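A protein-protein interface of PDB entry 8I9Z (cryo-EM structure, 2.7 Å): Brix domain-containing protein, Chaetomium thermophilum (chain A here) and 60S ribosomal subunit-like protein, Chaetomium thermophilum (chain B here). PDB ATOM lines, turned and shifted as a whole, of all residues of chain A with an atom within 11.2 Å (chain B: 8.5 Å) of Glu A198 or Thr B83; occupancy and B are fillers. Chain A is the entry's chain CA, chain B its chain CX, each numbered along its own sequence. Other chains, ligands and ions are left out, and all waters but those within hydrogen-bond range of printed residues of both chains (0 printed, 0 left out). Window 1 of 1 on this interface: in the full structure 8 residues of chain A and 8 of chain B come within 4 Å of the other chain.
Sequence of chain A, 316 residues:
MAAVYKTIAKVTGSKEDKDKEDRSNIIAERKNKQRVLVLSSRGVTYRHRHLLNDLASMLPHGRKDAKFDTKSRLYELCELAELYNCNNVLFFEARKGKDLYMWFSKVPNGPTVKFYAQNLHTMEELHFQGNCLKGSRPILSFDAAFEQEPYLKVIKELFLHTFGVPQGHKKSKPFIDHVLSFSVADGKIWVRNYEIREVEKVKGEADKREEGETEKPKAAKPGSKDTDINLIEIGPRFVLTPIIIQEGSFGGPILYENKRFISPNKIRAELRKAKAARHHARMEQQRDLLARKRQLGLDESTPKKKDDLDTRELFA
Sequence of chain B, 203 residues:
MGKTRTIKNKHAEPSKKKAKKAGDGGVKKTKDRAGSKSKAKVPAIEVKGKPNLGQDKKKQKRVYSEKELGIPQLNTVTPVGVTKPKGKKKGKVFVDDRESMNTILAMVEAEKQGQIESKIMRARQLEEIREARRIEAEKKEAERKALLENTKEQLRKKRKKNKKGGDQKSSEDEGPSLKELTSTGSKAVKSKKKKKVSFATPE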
ATOM      1  N   GLN A 129      31.543   2.981   9.766  1.00  0.00           N
ATOM      2  CA  GLN A 129      30.401   2.216   9.258  1.00  0.00           C
ATOM      3  C   GLN A 129      30.624   0.709   9.284  1.00  0.00           C
ATOM      4  O   GLN A 129      29.819  -0.033   8.713  1.00  0.00           O
ATOM      5  CB  GLN A 129      30.029   2.620   7.827  1.00  0.00           C
ATOM      6  CG  GLN A 129      29.795   4.089   7.630  1.00  0.00           C
ATOM      7  CD  GLN A 129      29.592   4.430   6.177  1.00  0.00           C
ATOM      8  OE1 GLN A 129      29.838   3.609   5.297  1.00  0.00           O
ATOM      9  NE2 GLN A 129      29.214   5.665   5.910  1.00  0.00           N
ATOM     10  N   ASN A 131      31.647  -3.011  11.473  1.00  0.00           N
ATOM     11  CA  ASN A 131      31.600  -3.692  12.755  1.00  0.00           C
ATOM     12  C   ASN A 131      31.856  -5.173  12.533  1.00  0.00           C
ATOM     13  O   ASN A 131      31.585  -5.708  11.456  1.00  0.00           O
ATOM     14  CB  ASN A 131      30.254  -3.483  13.450  1.00  0.00           C
ATOM     15  CG  ASN A 131      30.343  -3.614  14.949  1.00  0.00           C
ATOM     16  OD1 ASN A 131      31.323  -4.123  15.478  1.00  0.00           O
ATOM     17  ND2 ASN A 131      29.313  -3.160  15.645  1.00  0.00           N
ATOM     18  N   ILE A 139      41.831 -12.492   9.709  1.00  0.00           N
ATOM     19  CA  ILE A 139      42.785 -12.798   8.656  1.00  0.00           C
ATOM     20  C   ILE A 139      43.837 -11.702   8.685  1.00  0.00           C
ATOM     21  O   ILE A 139      43.508 -10.514   8.588  1.00  0.00           O
ATOM     22  CB  ILE A 139      42.104 -12.893   7.282  1.00  0.00           C
ATOM     23  CG1 ILE A 139      41.365 -14.224   7.147  1.00  0.00           C
ATOM     24  CG2 ILE A 139      43.123 -12.751   6.164  1.00  0.00           C
ATOM     25  CD1 ILE A 139      40.693 -14.415   5.815  1.00  0.00           C
ATOM     26  N   PHE A 175      33.129 -17.650  13.540  1.00  0.00           N
ATOM     27  CA  PHE A 175      32.994 -17.238  12.152  1.00  0.00           C
ATOM     28  C   PHE A 175      33.942 -16.085  11.858  1.00  0.00           C
ATOM     29  O   PHE A 175      34.410 -15.394  12.766  1.00  0.00           O
ATOM     30  CB  PHE A 175      31.544 -16.859  11.835  1.00  0.00           C
ATOM     31  CG  PHE A 175      30.571 -17.964  12.109  1.00  0.00           C
ATOM     32  CD1 PHE A 175      30.471 -19.041  11.251  1.00  0.00           C
ATOM     33  CD2 PHE A 175      29.778 -17.945  13.239  1.00  0.00           C
ATOM     34  CE1 PHE A 175      29.595 -20.064  11.505  1.00  0.00           C
ATOM     35  CE2 PHE A 175      28.900 -18.973  13.499  1.00  0.00           C
ATOM     36  CZ  PHE A 175      28.814 -20.034  12.630  1.00  0.00           C
ATOM     37  N   ILE A 176      34.230 -15.887  10.576  1.00  0.00           N
ATOM     38  CA  ILE A 176      35.245 -14.937  10.133  1.00  0.00           C
ATOM     39  C   ILE A 176      34.565 -13.775   9.426  1.00  0.00           C
ATOM     40  O   ILE A 176      33.870 -13.971   8.423  1.00  0.00           O
ATOM     41  CB  ILE A 176      36.274 -15.613   9.220  1.00  0.00           C
ATOM     42  CG1 ILE A 176      36.987 -16.716  10.006  1.00  0.00           C
ATOM     43  CG2 ILE A 176      37.230 -14.574   8.649  1.00  0.00           C
ATOM     44  CD1 ILE A 176      38.353 -17.060   9.518  1.00  0.00           C
ATOM     45  N   ASP A 177      34.776 -12.559   9.942  1.00  0.00           N
ATOM     46  CA  ASP A 177      34.149 -11.385   9.351  1.00  0.00           C
ATOM     47  C   ASP A 177      35.051 -10.157   9.296  1.00  0.00           C
ATOM     48  O   ASP A 177      34.575  -9.088   8.893  1.00  0.00           O
ATOM     49  CB  ASP A 177      32.864 -11.022  10.100  1.00  0.00           C
ATOM     50  CG  ASP A 177      33.039 -11.029  11.600  1.00  0.00           C
ATOM     51  OD1 ASP A 177      34.176 -11.227  12.070  1.00  0.00           O
ATOM     52  OD2 ASP A 177      32.033 -10.837  12.310  1.00  0.00           O
ATOM     53  N   HIS A 178      36.323 -10.250   9.679  1.00  0.00           N
ATOM     54  CA  HIS A 178      37.171  -9.072   9.603  1.00  0.00           C
ATOM     55  C   HIS A 178      38.613  -9.460   9.321  1.00  0.00           C
ATOM     56  O   HIS A 178      39.053 -10.567   9.637  1.00  0.00           O
ATOM     57  CB  HIS A 178      37.066  -8.215  10.873  1.00  0.00           C
ATOM     58  CG  HIS A 178      37.939  -8.659  12.004  1.00  0.00           C
ATOM     59  ND1 HIS A 178      37.594  -9.686  12.853  1.00  0.00           N
ATOM     60  CD2 HIS A 178      39.125  -8.184  12.451  1.00  0.00           C
ATOM     61  CE1 HIS A 178      38.537  -9.837  13.765  1.00  0.00           C
ATOM     62  NE2 HIS A 178      39.477  -8.937  13.542  1.00  0.00           N
ATOM     63  N   VAL A 179      39.339  -8.524   8.714  1.00  0.00           N
ATOM     64  CA  VAL A 179      40.724  -8.711   8.304  1.00  0.00           C
ATOM     65  C   VAL A 179      41.542  -7.544   8.836  1.00  0.00           C
ATOM     66  O   VAL A 179      41.169  -6.381   8.653  1.00  0.00           O
ATOM     67  CB  VAL A 179      40.850  -8.827   6.769  1.00  0.00           C
ATOM     68  CG1 VAL A 179      39.844  -7.926   6.077  1.00  0.00           C
ATOM     69  CG2 VAL A 179      42.256  -8.500   6.301  1.00  0.00           C
ATOM     70  N   TYR A 194      39.311  -4.023   8.476  1.00  0.00           N
ATOM     71  CA  TYR A 194      38.279  -4.028   7.454  1.00  0.00           C
ATOM     72  C   TYR A 194      37.268  -5.123   7.747  1.00  0.00           C
ATOM     73  O   TYR A 194      37.596  -6.142   8.350  1.00  0.00           O
ATOM     74  CB  TYR A 194      38.875  -4.222   6.057  1.00  0.00           C
ATOM     75  CG  TYR A 194      39.865  -3.152   5.662  1.00  0.00           C
ATOM     76  CD1 TYR A 194      39.453  -1.848   5.443  1.00  0.00           C
ATOM     77  CD2 TYR A 194      41.212  -3.443   5.526  1.00  0.00           C
ATOM     78  CE1 TYR A 194      40.351  -0.870   5.094  1.00  0.00           C
ATOM     79  CE2 TYR A 194      42.115  -2.470   5.169  1.00  0.00           C
ATOM     80  CZ  TYR A 194      41.677  -1.184   4.954  1.00  0.00           C
ATOM     81  OH  TYR A 194      42.574  -0.204   4.603  1.00  0.00           O
ATOM     82  N   GLU A 195      36.035  -4.905   7.306  1.00  0.00           N
ATOM     83  CA  GLU A 195      34.964  -5.873   7.485  1.00  0.00           C
ATOM     84  C   GLU A 195      34.745  -6.643   6.194  1.00  0.00           C
ATOM     85  O   GLU A 195      34.593  -6.045   5.127  1.00  0.00           O
ATOM     86  CB  GLU A 195      33.671  -5.178   7.903  1.00  0.00           C
ATOM     87  CG  GLU A 195      32.554  -6.120   8.279  1.00  0.00           C
ATOM     88  CD  GLU A 195      31.195  -5.474   8.154  1.00  0.00           C
ATOM     89  OE1 GLU A 195      31.113  -4.239   8.307  1.00  0.00           O
ATOM     90  OE2 GLU A 195      30.206  -6.196   7.913  1.00  0.00           O
ATOM     91  N   ILE A 196      34.727  -7.970   6.293  1.00  0.00           N
ATOM     92  CA  ILE A 196      34.438  -8.816   5.142  1.00  0.00           C
ATOM     93  C   ILE A 196      32.922  -8.825   4.970  1.00  0.00           C
ATOM     94  O   ILE A 196      32.198  -9.461   5.735  1.00  0.00           O
ATOM     95  CB  ILE A 196      35.008 -10.225   5.307  1.00  0.00           C
ATOM     96  CG1 ILE A 196      36.530 -10.187   5.198  1.00  0.00           C
ATOM     97  CG2 ILE A 196      34.475 -11.152   4.225  1.00  0.00           C
ATOM     98  CD1 ILE A 196      37.232 -11.130   6.139  1.00  0.00           C
ATOM     99  N   ARG A 197      32.437  -8.081   3.982  1.00  0.00           N
ATOM    100  CA  ARG A 197      31.016  -7.997   3.675  1.00  0.00           C
ATOM    101  C   ARG A 197      30.758  -8.745   2.374  1.00  0.00           C
ATOM    102  O   ARG A 197      31.393  -8.459   1.353  1.00  0.00           O
ATOM    103  CB  ARG A 197      30.568  -6.540   3.571  1.00  0.00           C
ATOM    104  CG  ARG A 197      29.305  -6.324   2.763  1.00  0.00           C
ATOM    105  CD  ARG A 197      28.067  -6.421   3.627  1.00  0.00           C
ATOM    106  NE  ARG A 197      28.157  -5.586   4.817  1.00  0.00           N
ATOM    107  CZ  ARG A 197      27.527  -4.431   4.968  1.00  0.00           C
ATOM    108  NH1 ARG A 197      26.761  -3.932   4.014  1.00  0.00           N
ATOM    109  NH2 ARG A 197      27.673  -3.757   6.105  1.00  0.00           N
ATOM    110  N   GLU A 198      29.838  -9.704   2.413  1.00  0.00           N
ATOM    111  CA  GLU A 198      29.577 -10.566   1.272  1.00  0.00           C
ATOM    112  C   GLU A 198      28.380 -10.054   0.486  1.00  0.00           C
ATOM    113  O   GLU A 198      27.320  -9.785   1.058  1.00  0.00           O
ATOM    114  CB  GLU A 198      29.342 -12.004   1.727  1.00  0.00           C
ATOM    115  CG  GLU A 198      30.614 -12.753   2.062  1.00  0.00           C
ATOM    116  CD  GLU A 198      30.344 -14.128   2.624  1.00  0.00           C
ATOM    117  OE1 GLU A 198      29.178 -14.407   2.963  1.00  0.00           O
ATOM    118  OE2 GLU A 198      31.296 -14.931   2.725  1.00  0.00           O
ATOM    119  N   VAL A 199      28.558  -9.916  -0.824  1.00  0.00           N
ATOM    120  CA  VAL A 199      27.542  -9.394  -1.728  1.00  0.00           C
ATOM    121  C   VAL A 199      27.268 -10.453  -2.784  1.00  0.00           C
ATOM    122  O   VAL A 199      28.206 -11.053  -3.320  1.00  0.00           O
ATOM    123  CB  VAL A 199      27.994  -8.069  -2.370  1.00  0.00           C
ATOM    124  CG1 VAL A 199      26.967  -7.562  -3.365  1.00  0.00           C
ATOM    125  CG2 VAL A 199      28.256  -7.026  -1.302  1.00  0.00           C
ATOM    126  N   GLU A 200      25.988 -10.709  -3.051  1.00  0.00           N
ATOM    127  CA  GLU A 200      25.603 -11.689  -4.058  1.00  0.00           C
ATOM    128  C   GLU A 200      26.072 -11.250  -5.438  1.00  0.00           C
ATOM    129  O   GLU A 200      25.927 -10.086  -5.816  1.00  0.00           O
ATOM    130  CB  GLU A 200      24.089 -11.883  -4.048  1.00  0.00           C
ATOM    131  CG  GLU A 200      23.603 -12.905  -3.039  1.00  0.00           C
ATOM    132  CD  GLU A 200      22.336 -13.606  -3.483  1.00  0.00           C
ATOM    133  OE1 GLU A 200      21.979 -13.493  -4.675  1.00  0.00           O
ATOM    134  OE2 GLU A 200      21.695 -14.269  -2.641  1.00  0.00           O
ATOM    135  N   LYS A 201      26.651 -12.186  -6.185  1.00  0.00           N
ATOM    136  CA  LYS A 201      27.210 -11.860  -7.488  1.00  0.00           C
ATOM    137  C   LYS A 201      26.104 -11.662  -8.512  1.00  0.00           C
ATOM    138  O   LYS A 201      25.082 -12.354  -8.492  1.00  0.00           O
ATOM    139  CB  LYS A 201      28.157 -12.966  -7.948  1.00  0.00           C
ATOM    140  CG  LYS A 201      29.569 -12.834  -7.415  1.00  0.00           C
ATOM    141  CD  LYS A 201      30.467 -13.924  -7.969  1.00  0.00           C
ATOM    142  CE  LYS A 201      31.841 -13.381  -8.315  1.00  0.00           C
ATOM    143  NZ  LYS A 201      31.758 -12.176  -9.183  1.00  0.00           N
ATOM    144  N   VAL A 202      26.311 -10.709  -9.413  1.00  0.00           N
ATOM    145  CA  VAL A 202      25.364 -10.466 -10.494  1.00  0.00           C
ATOM    146  C   VAL A 202      25.578 -11.511 -11.579  1.00  0.00           C
ATOM    147  O   VAL A 202      26.706 -11.730 -12.034  1.00  0.00           O
ATOM    148  CB  VAL A 202      25.526  -9.044 -11.052  1.00  0.00           C
ATOM    149  CG1 VAL A 202      24.415  -8.736 -12.040  1.00  0.00           C
ATOM    150  CG2 VAL A 202      25.532  -8.032  -9.918  1.00  0.00           C
ATOM    151  N   THR A 227      29.497 -15.503  -4.517  1.00  0.00           N
ATOM    152  CA  THR A 227      29.460 -14.232  -3.803  1.00  0.00           C
ATOM    153  C   THR A 227      30.824 -13.552  -3.811  1.00  0.00           C
ATOM    154  O   THR A 227      31.858 -14.213  -3.869  1.00  0.00           O
ATOM    155  CB  THR A 227      28.989 -14.421  -2.349  1.00  0.00           C
ATOM    156  OG1 THR A 227      29.161 -13.200  -1.625  1.00  0.00           O
ATOM    157  CG2 THR A 227      29.768 -15.530  -1.668  1.00  0.00           C
ATOM    158  N   ASP A 228      30.821 -12.226  -3.763  1.00  0.00           N
ATOM    159  CA  ASP A 228      32.038 -11.430  -3.752  1.00  0.00           C
ATOM    160  C   ASP A 228      32.193 -10.728  -2.408  1.00  0.00           C
ATOM    161  O   ASP A 228      31.298 -10.750  -1.560  1.00  0.00           O
ATOM    162  CB  ASP A 228      32.035 -10.415  -4.901  1.00  0.00           C
ATOM    163  CG  ASP A 228      30.817  -9.514  -4.882  1.00  0.00           C
ATOM    164  OD1 ASP A 228      30.829  -8.507  -4.142  1.00  0.00           O
ATOM    165  OD2 ASP A 228      29.846  -9.811  -5.608  1.00  0.00           O
ATOM    166  N   ILE A 229      33.347 -10.095  -2.222  1.00  0.00           N
ATOM    167  CA  ILE A 229      33.731  -9.506  -0.946  1.00  0.00           C
ATOM    168  C   ILE A 229      33.926  -8.007  -1.123  1.00  0.00           C
ATOM    169  O   ILE A 229      34.628  -7.566  -2.039  1.00  0.00           O
ATOM    170  CB  ILE A 229      35.019 -10.155  -0.396  1.00  0.00           C
ATOM    171  CG1 ILE A 229      34.766 -11.607  -0.006  1.00  0.00           C
ATOM    172  CG2 ILE A 229      35.553  -9.392   0.802  1.00  0.00           C
ATOM    173  CD1 ILE A 229      36.030 -12.366   0.303  1.00  0.00           C
ATOM    174  N   ASN A 230      33.297  -7.227  -0.250  1.00  0.00           N
ATOM    175  CA  ASN A 230      33.573  -5.808  -0.108  1.00  0.00           C
ATOM    176  C   ASN A 230      34.170  -5.557   1.270  1.00  0.00           C
ATOM    177  O   ASN A 230      33.844  -6.251   2.237  1.00  0.00           O
ATOM    178  CB  ASN A 230      32.308  -4.969  -0.292  1.00  0.00           C
ATOM    179  CG  ASN A 230      31.941  -4.786  -1.744  1.00  0.00           C
ATOM    180  OD1 ASN A 230      32.517  -5.421  -2.625  1.00  0.00           O
ATOM    181  ND2 ASN A 230      30.974  -3.914  -2.005  1.00  0.00           N
ATOM    182  N   LEU A 231      35.051  -4.567   1.358  1.00  0.00           N
ATOM    183  CA  LEU A 231      35.723  -4.225   2.603  1.00  0.00           C
ATOM    184  C   LEU A 231      35.202  -2.895   3.126  1.00  0.00           C
ATOM    185  O   LEU A 231      35.217  -1.892   2.409  1.00  0.00           O
ATOM    186  CB  LEU A 231      37.236  -4.152   2.407  1.00  0.00           C
ATOM    187  CG  LEU A 231      37.999  -5.470   2.316  1.00  0.00           C
ATOM    188  CD1 LEU A 231      39.480  -5.226   2.523  1.00  0.00           C
ATOM    189  CD2 LEU A 231      37.480  -6.475   3.325  1.00  0.00           C
ATOM    190  N   ILE A 232      34.744  -2.894   4.373  1.00  0.00           N
ATOM    191  CA  ILE A 232      34.326  -1.685   5.072  1.00  0.00           C
ATOM    192  C   ILE A 232      35.210  -1.538   6.300  1.00  0.00           C
ATOM    193  O   ILE A 232      35.362  -2.488   7.078  1.00  0.00           O
ATOM    194  CB  ILE A 232      32.843  -1.722   5.467  1.00  0.00           C
ATOM    195  CG1 ILE A 232      31.992  -2.249   4.316  1.00  0.00           C
ATOM    196  CG2 ILE A 232      32.370  -0.341   5.878  1.00  0.00           C
ATOM    197  CD1 ILE A 232      30.581  -2.578   4.713  1.00  0.00           C
ATOM    198  N   PRO B  72      23.633   2.711   3.578  1.00  0.00           N
ATOM    199  CA  PRO B  72      24.211   1.365   3.632  1.00  0.00           C
ATOM    200  C   PRO B  72      23.724   0.597   4.849  1.00  0.00           C
ATOM    201  O   PRO B  72      23.358   1.173   5.874  1.00  0.00           O
ATOM    202  CB  PRO B  72      25.719   1.628   3.719  1.00  0.00           C
ATOM    203  CG  PRO B  72      25.895   3.061   3.316  1.00  0.00           C
ATOM    204  CD  PRO B  72      24.655   3.752   3.754  1.00  0.00           C
ATOM    205  N   GLN B  73      23.718  -0.725   4.720  1.00  0.00           N
ATOM    206  CA  GLN B  73      23.357  -1.589   5.833  1.00  0.00           C
ATOM    207  C   GLN B  73      24.534  -1.736   6.784  1.00  0.00           C
ATOM    208  O   GLN B  73      25.680  -1.895   6.356  1.00  0.00           O
ATOM    209  CB  GLN B  73      22.911  -2.959   5.328  1.00  0.00           C
ATOM    210  CG  GLN B  73      22.197  -2.919   3.994  1.00  0.00           C
ATOM    211  CD  GLN B  73      21.228  -4.066   3.824  1.00  0.00           C
ATOM    212  OE1 GLN B  73      20.132  -4.052   4.379  1.00  0.00           O
ATOM    213  NE2 GLN B  73      21.625  -5.065   3.050  1.00  0.00           N
ATOM    214  N   LEU B  74      24.247  -1.690   8.080  1.00  0.00           N
ATOM    215  CA  LEU B  74      25.270  -1.658   9.113  1.00  0.00           C
ATOM    216  C   LEU B  74      25.238  -2.940   9.928  1.00  0.00           C
ATOM    217  O   LEU B  74      24.165  -3.418  10.309  1.00  0.00           O
ATOM    218  CB  LEU B  74      25.077  -0.452  10.031  1.00  0.00           C
ATOM    219  CG  LEU B  74      25.276   0.904   9.357  1.00  0.00           C
ATOM    220  CD1 LEU B  74      24.829   2.014  10.277  1.00  0.00           C
ATOM    221  CD2 LEU B  74      26.722   1.098   8.948  1.00  0.00           C
ATOM    222  N   ASN B  75      26.418  -3.490  10.203  1.00  0.00           N
ATOM    223  CA  ASN B  75      26.538  -4.750  10.931  1.00  0.00           C
ATOM    224  C   ASN B  75      26.347  -4.475  12.415  1.00  0.00           C
ATOM    225  O   ASN B  75      27.054  -3.661  13.009  1.00  0.00           O
ATOM    226  CB  ASN B  75      27.881  -5.411  10.652  1.00  0.00           C
ATOM    227  CG  ASN B  75      27.877  -6.887  10.972  1.00  0.00           C
ATOM    228  OD1 ASN B  75      26.860  -7.442  11.378  1.00  0.00           O
ATOM    229  ND2 ASN B  75      29.019  -7.535  10.789  1.00  0.00           N
ATOM    230  N   PRO B  79      22.747  -9.652  12.461  1.00  0.00           N
ATOM    231  CA  PRO B  79      23.700  -9.667  11.346  1.00  0.00           C
ATOM    232  C   PRO B  79      23.118  -9.104  10.062  1.00  0.00           C
ATOM    233  O   PRO B  79      21.905  -9.112   9.841  1.00  0.00           O
ATOM    234  CB  PRO B  79      24.038 -11.152  11.191  1.00  0.00           C
ATOM    235  CG  PRO B  79      22.902 -11.857  11.787  1.00  0.00           C
ATOM    236  CD  PRO B  79      22.371 -11.008  12.883  1.00  0.00           C
ATOM    237  N   VAL B  80      24.012  -8.612   9.204  1.00  0.00           N
ATOM    238  CA  VAL B  80      23.587  -8.100   7.908  1.00  0.00           C
ATOM    239  C   VAL B  80      23.311  -9.229   6.929  1.00  0.00           C
ATOM    240  O   VAL B  80      22.401  -9.122   6.101  1.00  0.00           O
ATOM    241  CB  VAL B  80      24.626  -7.118   7.339  1.00  0.00           C
ATOM    242  CG1 VAL B  80      24.505  -5.786   8.021  1.00  0.00           C
ATOM    243  CG2 VAL B  80      26.028  -7.664   7.519  1.00  0.00           C
ATOM    244  N   GLY B  81      24.073 -10.312   6.997  1.00  0.00           N
ATOM    245  CA  GLY B  81      23.922 -11.367   6.028  1.00  0.00           C
ATOM    246  C   GLY B  81      24.499 -10.957   4.684  1.00  0.00           C
ATOM    247  O   GLY B  81      25.181  -9.941   4.544  1.00  0.00           O
ATOM    248  N   VAL B  82      24.210 -11.775   3.681  1.00  0.00           N
ATOM    249  CA  VAL B  82      24.634 -11.480   2.320  1.00  0.00           C
ATOM    250  C   VAL B  82      23.705 -10.426   1.742  1.00  0.00           C
ATOM    251  O   VAL B  82      22.481 -10.596   1.738  1.00  0.00           O
ATOM    252  CB  VAL B  82      24.639 -12.755   1.463  1.00  0.00           C
ATOM    253  CG1 VAL B  82      25.554 -12.582   0.265  1.00  0.00           C
ATOM    254  CG2 VAL B  82      25.072 -13.944   2.296  1.00  0.00           C
ATOM    255  N   THR B  83      24.280  -9.333   1.258  1.00  0.00           N
ATOM    256  CA  THR B  83      23.514  -8.189   0.784  1.00  0.00           C
ATOM    257  C   THR B  83      23.403  -8.249  -0.733  1.00  0.00           C
ATOM    258  O   THR B  83      24.417  -8.345  -1.430  1.00  0.00           O
ATOM    259  CB  THR B  83      24.165  -6.879   1.220  1.00  0.00           C
ATOM    260  OG1 THR B  83      25.390  -6.692   0.501  1.00  0.00           O
ATOM    261  CG2 THR B  83      24.465  -6.909   2.708  1.00  0.00           C
ATOM    262  N   LYS B  84      22.186  -8.200  -1.234  1.00  0.00           N
ATOM    263  CA  LYS B  84      21.965  -8.217  -2.671  1.00  0.00           C
ATOM    264  C   LYS B  84      22.246  -6.838  -3.265  1.00  0.00           C
ATOM    265  O   LYS B  84      21.962  -5.821  -2.629  1.00  0.00           O
ATOM    266  CB  LYS B  84      20.537  -8.646  -2.982  1.00  0.00           C
ATOM    267  CG  LYS B  84      20.240 -10.072  -2.562  1.00  0.00           C
ATOM    268  CD  LYS B  84      18.918 -10.170  -1.842  1.00  0.00           C
ATOM    269  CE  LYS B  84      18.222 -11.476  -2.161  1.00  0.00           C
ATOM    270  NZ  LYS B  84      19.174 -12.618  -2.143  1.00  0.00           N
ATOM    271  N   PRO B  85      22.820  -6.778  -4.469  1.00  0.00           N
ATOM    272  CA  PRO B  85      23.147  -5.480  -5.073  1.00  0.00           C
ATOM    273  C   PRO B  85      21.905  -4.680  -5.435  1.00  0.00           C
ATOM    274  O   PRO B  85      20.837  -5.232  -5.706  1.00  0.00           O
ATOM    275  CB  PRO B  85      23.938  -5.860  -6.326  1.00  0.00           C
ATOM    276  CG  PRO B  85      24.412  -7.233  -6.073  1.00  0.00           C
ATOM    277  CD  PRO B  85      23.364  -7.896  -5.249  1.00  0.00           C
ATOM    278  N   LYS B  86      22.062  -3.361  -5.437  1.00  0.00           N
ATOM    279  CA  LYS B  86      20.970  -2.451  -5.738  1.00  0.00           C
ATOM    280  C   LYS B  86      20.760  -2.360  -7.241  1.00  0.00           C
ATOM    281  O   LYS B  86      21.722  -2.321  -8.014  1.00  0.00           O
ATOM    282  CB  LYS B  86      21.256  -1.065  -5.162  1.00  0.00           C
ATOM    283  CG  LYS B  86      20.085  -0.103  -5.237  1.00  0.00           C
ATOM    284  CD  LYS B  86      20.542   1.336  -5.050  1.00  0.00           C
ATOM    285  CE  LYS B  86      20.093   2.217  -6.205  1.00  0.00           C
ATOM    286  NZ  LYS B  86      18.857   1.701  -6.857  1.00  0.00           N
ATOM    287  N   LYS B  90      16.681  -9.212  -7.159  1.00  0.00           N
ATOM    288  CA  LYS B  90      16.511  -9.774  -5.821  1.00  0.00           C
ATOM    289  C   LYS B  90      15.654 -11.032  -5.936  1.00  0.00           C
ATOM    290  O   LYS B  90      14.422 -10.987  -5.918  1.00  0.00           O
ATOM    291  CB  LYS B  90      15.879  -8.753  -4.884  1.00  0.00           C
ATOM    292  CG  LYS B  90      16.782  -7.590  -4.525  1.00  0.00           C
ATOM    293  CD  LYS B  90      16.337  -6.901  -3.239  1.00  0.00           C
ATOM    294  CE  LYS B  90      14.891  -6.426  -3.288  1.00  0.00           C
ATOM    295  NZ  LYS B  90      14.530  -5.773  -4.576  1.00  0.00           N
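O of Gln B73 is in hydrogen-bond range of NH2 of Arg A197 (2.7 Å). The backbone carbonyl oxygen (O) of Asn A131 is in hydrogen-bond range of the side-chain amide nitrogen (ND2) of Asn B75, at 3.2 Å. OE2 of Glu A195 sits at hydrogen-bond distance from ND2 of Asn B75 (3.4 Å). The backbone carbonyl oxygen (O) of Glu A198 sits at hydrogen-bond distance from the backbone NH (N) of Thr B83 (3.1 Å). The backbone carbonyl oxygen (O) of Thr B83 is in hydrogen-bond range of the backbone NH (N) of Glu A200 (3.3 Å). The side-chain carboxylate (OE2) of Glu A200 is in salt-bridge range of the side-chain amino group (NZ) of Lys B84 (3.1 Å).
The side-chain carboxylate (OE1) of Glu A195 is in hydrogen-bond range of the backbone NH (N) of Asn A131, at 3.4 Å. The side-chain carboxylate (OE2) of Glu A195 lies within salt-bridge range of the guanidinium group (NE) of Arg A197. The backbone NH (N) of Glu A195 sits at hydrogen-bond distance from the backbone carbonyl oxygen (O) of Ile A232, at 2.5 Å. The backbone carbonyl oxygen of Arg A197 sits at hydrogen-bond distance from the backbone NH of Asn A230, 2.8 Å away. The side-chain hydroxyl (OG1) of Thr A227 lies within hydrogen-bond range of the backbone carbonyl oxygen (O) of Val A199 (2.9 Å). The backbone NH (N) of Asp A228 is in hydrogen-bond range of the backbone carbonyl oxygen (O) of Val A199, at 2.9 Å.
Among the printed residues, merely in contact across the chains: Gln A129 with Leu B74, Arg A197 with Thr B83, Glu A198 with Val B82, Val A199 with Thr B83, Val A199 with Pro B85, Glu A200 with Val B82 and Glu A200 with Pro B85.
Of the printed residues of chain B, Glu A198 touches Val B82 (3.4 Å) and Thr B83 (3.1 Å). Thr B83 touches four residues of chain A. No residue of chain A comes within 4 Å of Gly B81. Val B82 touches just these residues of chain A: Glu A198 and Glu A200. Pro B85 touches two residues of chain A. Printed residues of chain B within 4 Å of Arg A197: Gln B73 and Thr B83. Printed residues of chain B within 4 Å of Glu A195: Asn B75 (3.4 Å). Thr A227 touches none of the printed residues of chain B. The nearest printed residue of chain B that does not touch Glu A195 is Val B80 (4.4 Å).
Of the 13 printed residues of chain B, 7 touch a printed residue of chain A. Hydrophobic or aromatic side chains of chain B within 4 Å of the printed part of chain A: Leu B74, Val B82 and Pro B85. Of the 23 printed residues of chain A, 7 touch a printed residue of chain B. Hydrophobic or aromatic side chains of chain A within 4 Å of the printed part of chain B: Val A199. Among the printed residues, 13 pairs touch across the chains. Among the printed residues, Asp or Glu carboxylates within 4 Å of a Lys or Arg side-chain nitrogen of the other chain: Glu A200 with Lys B84.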
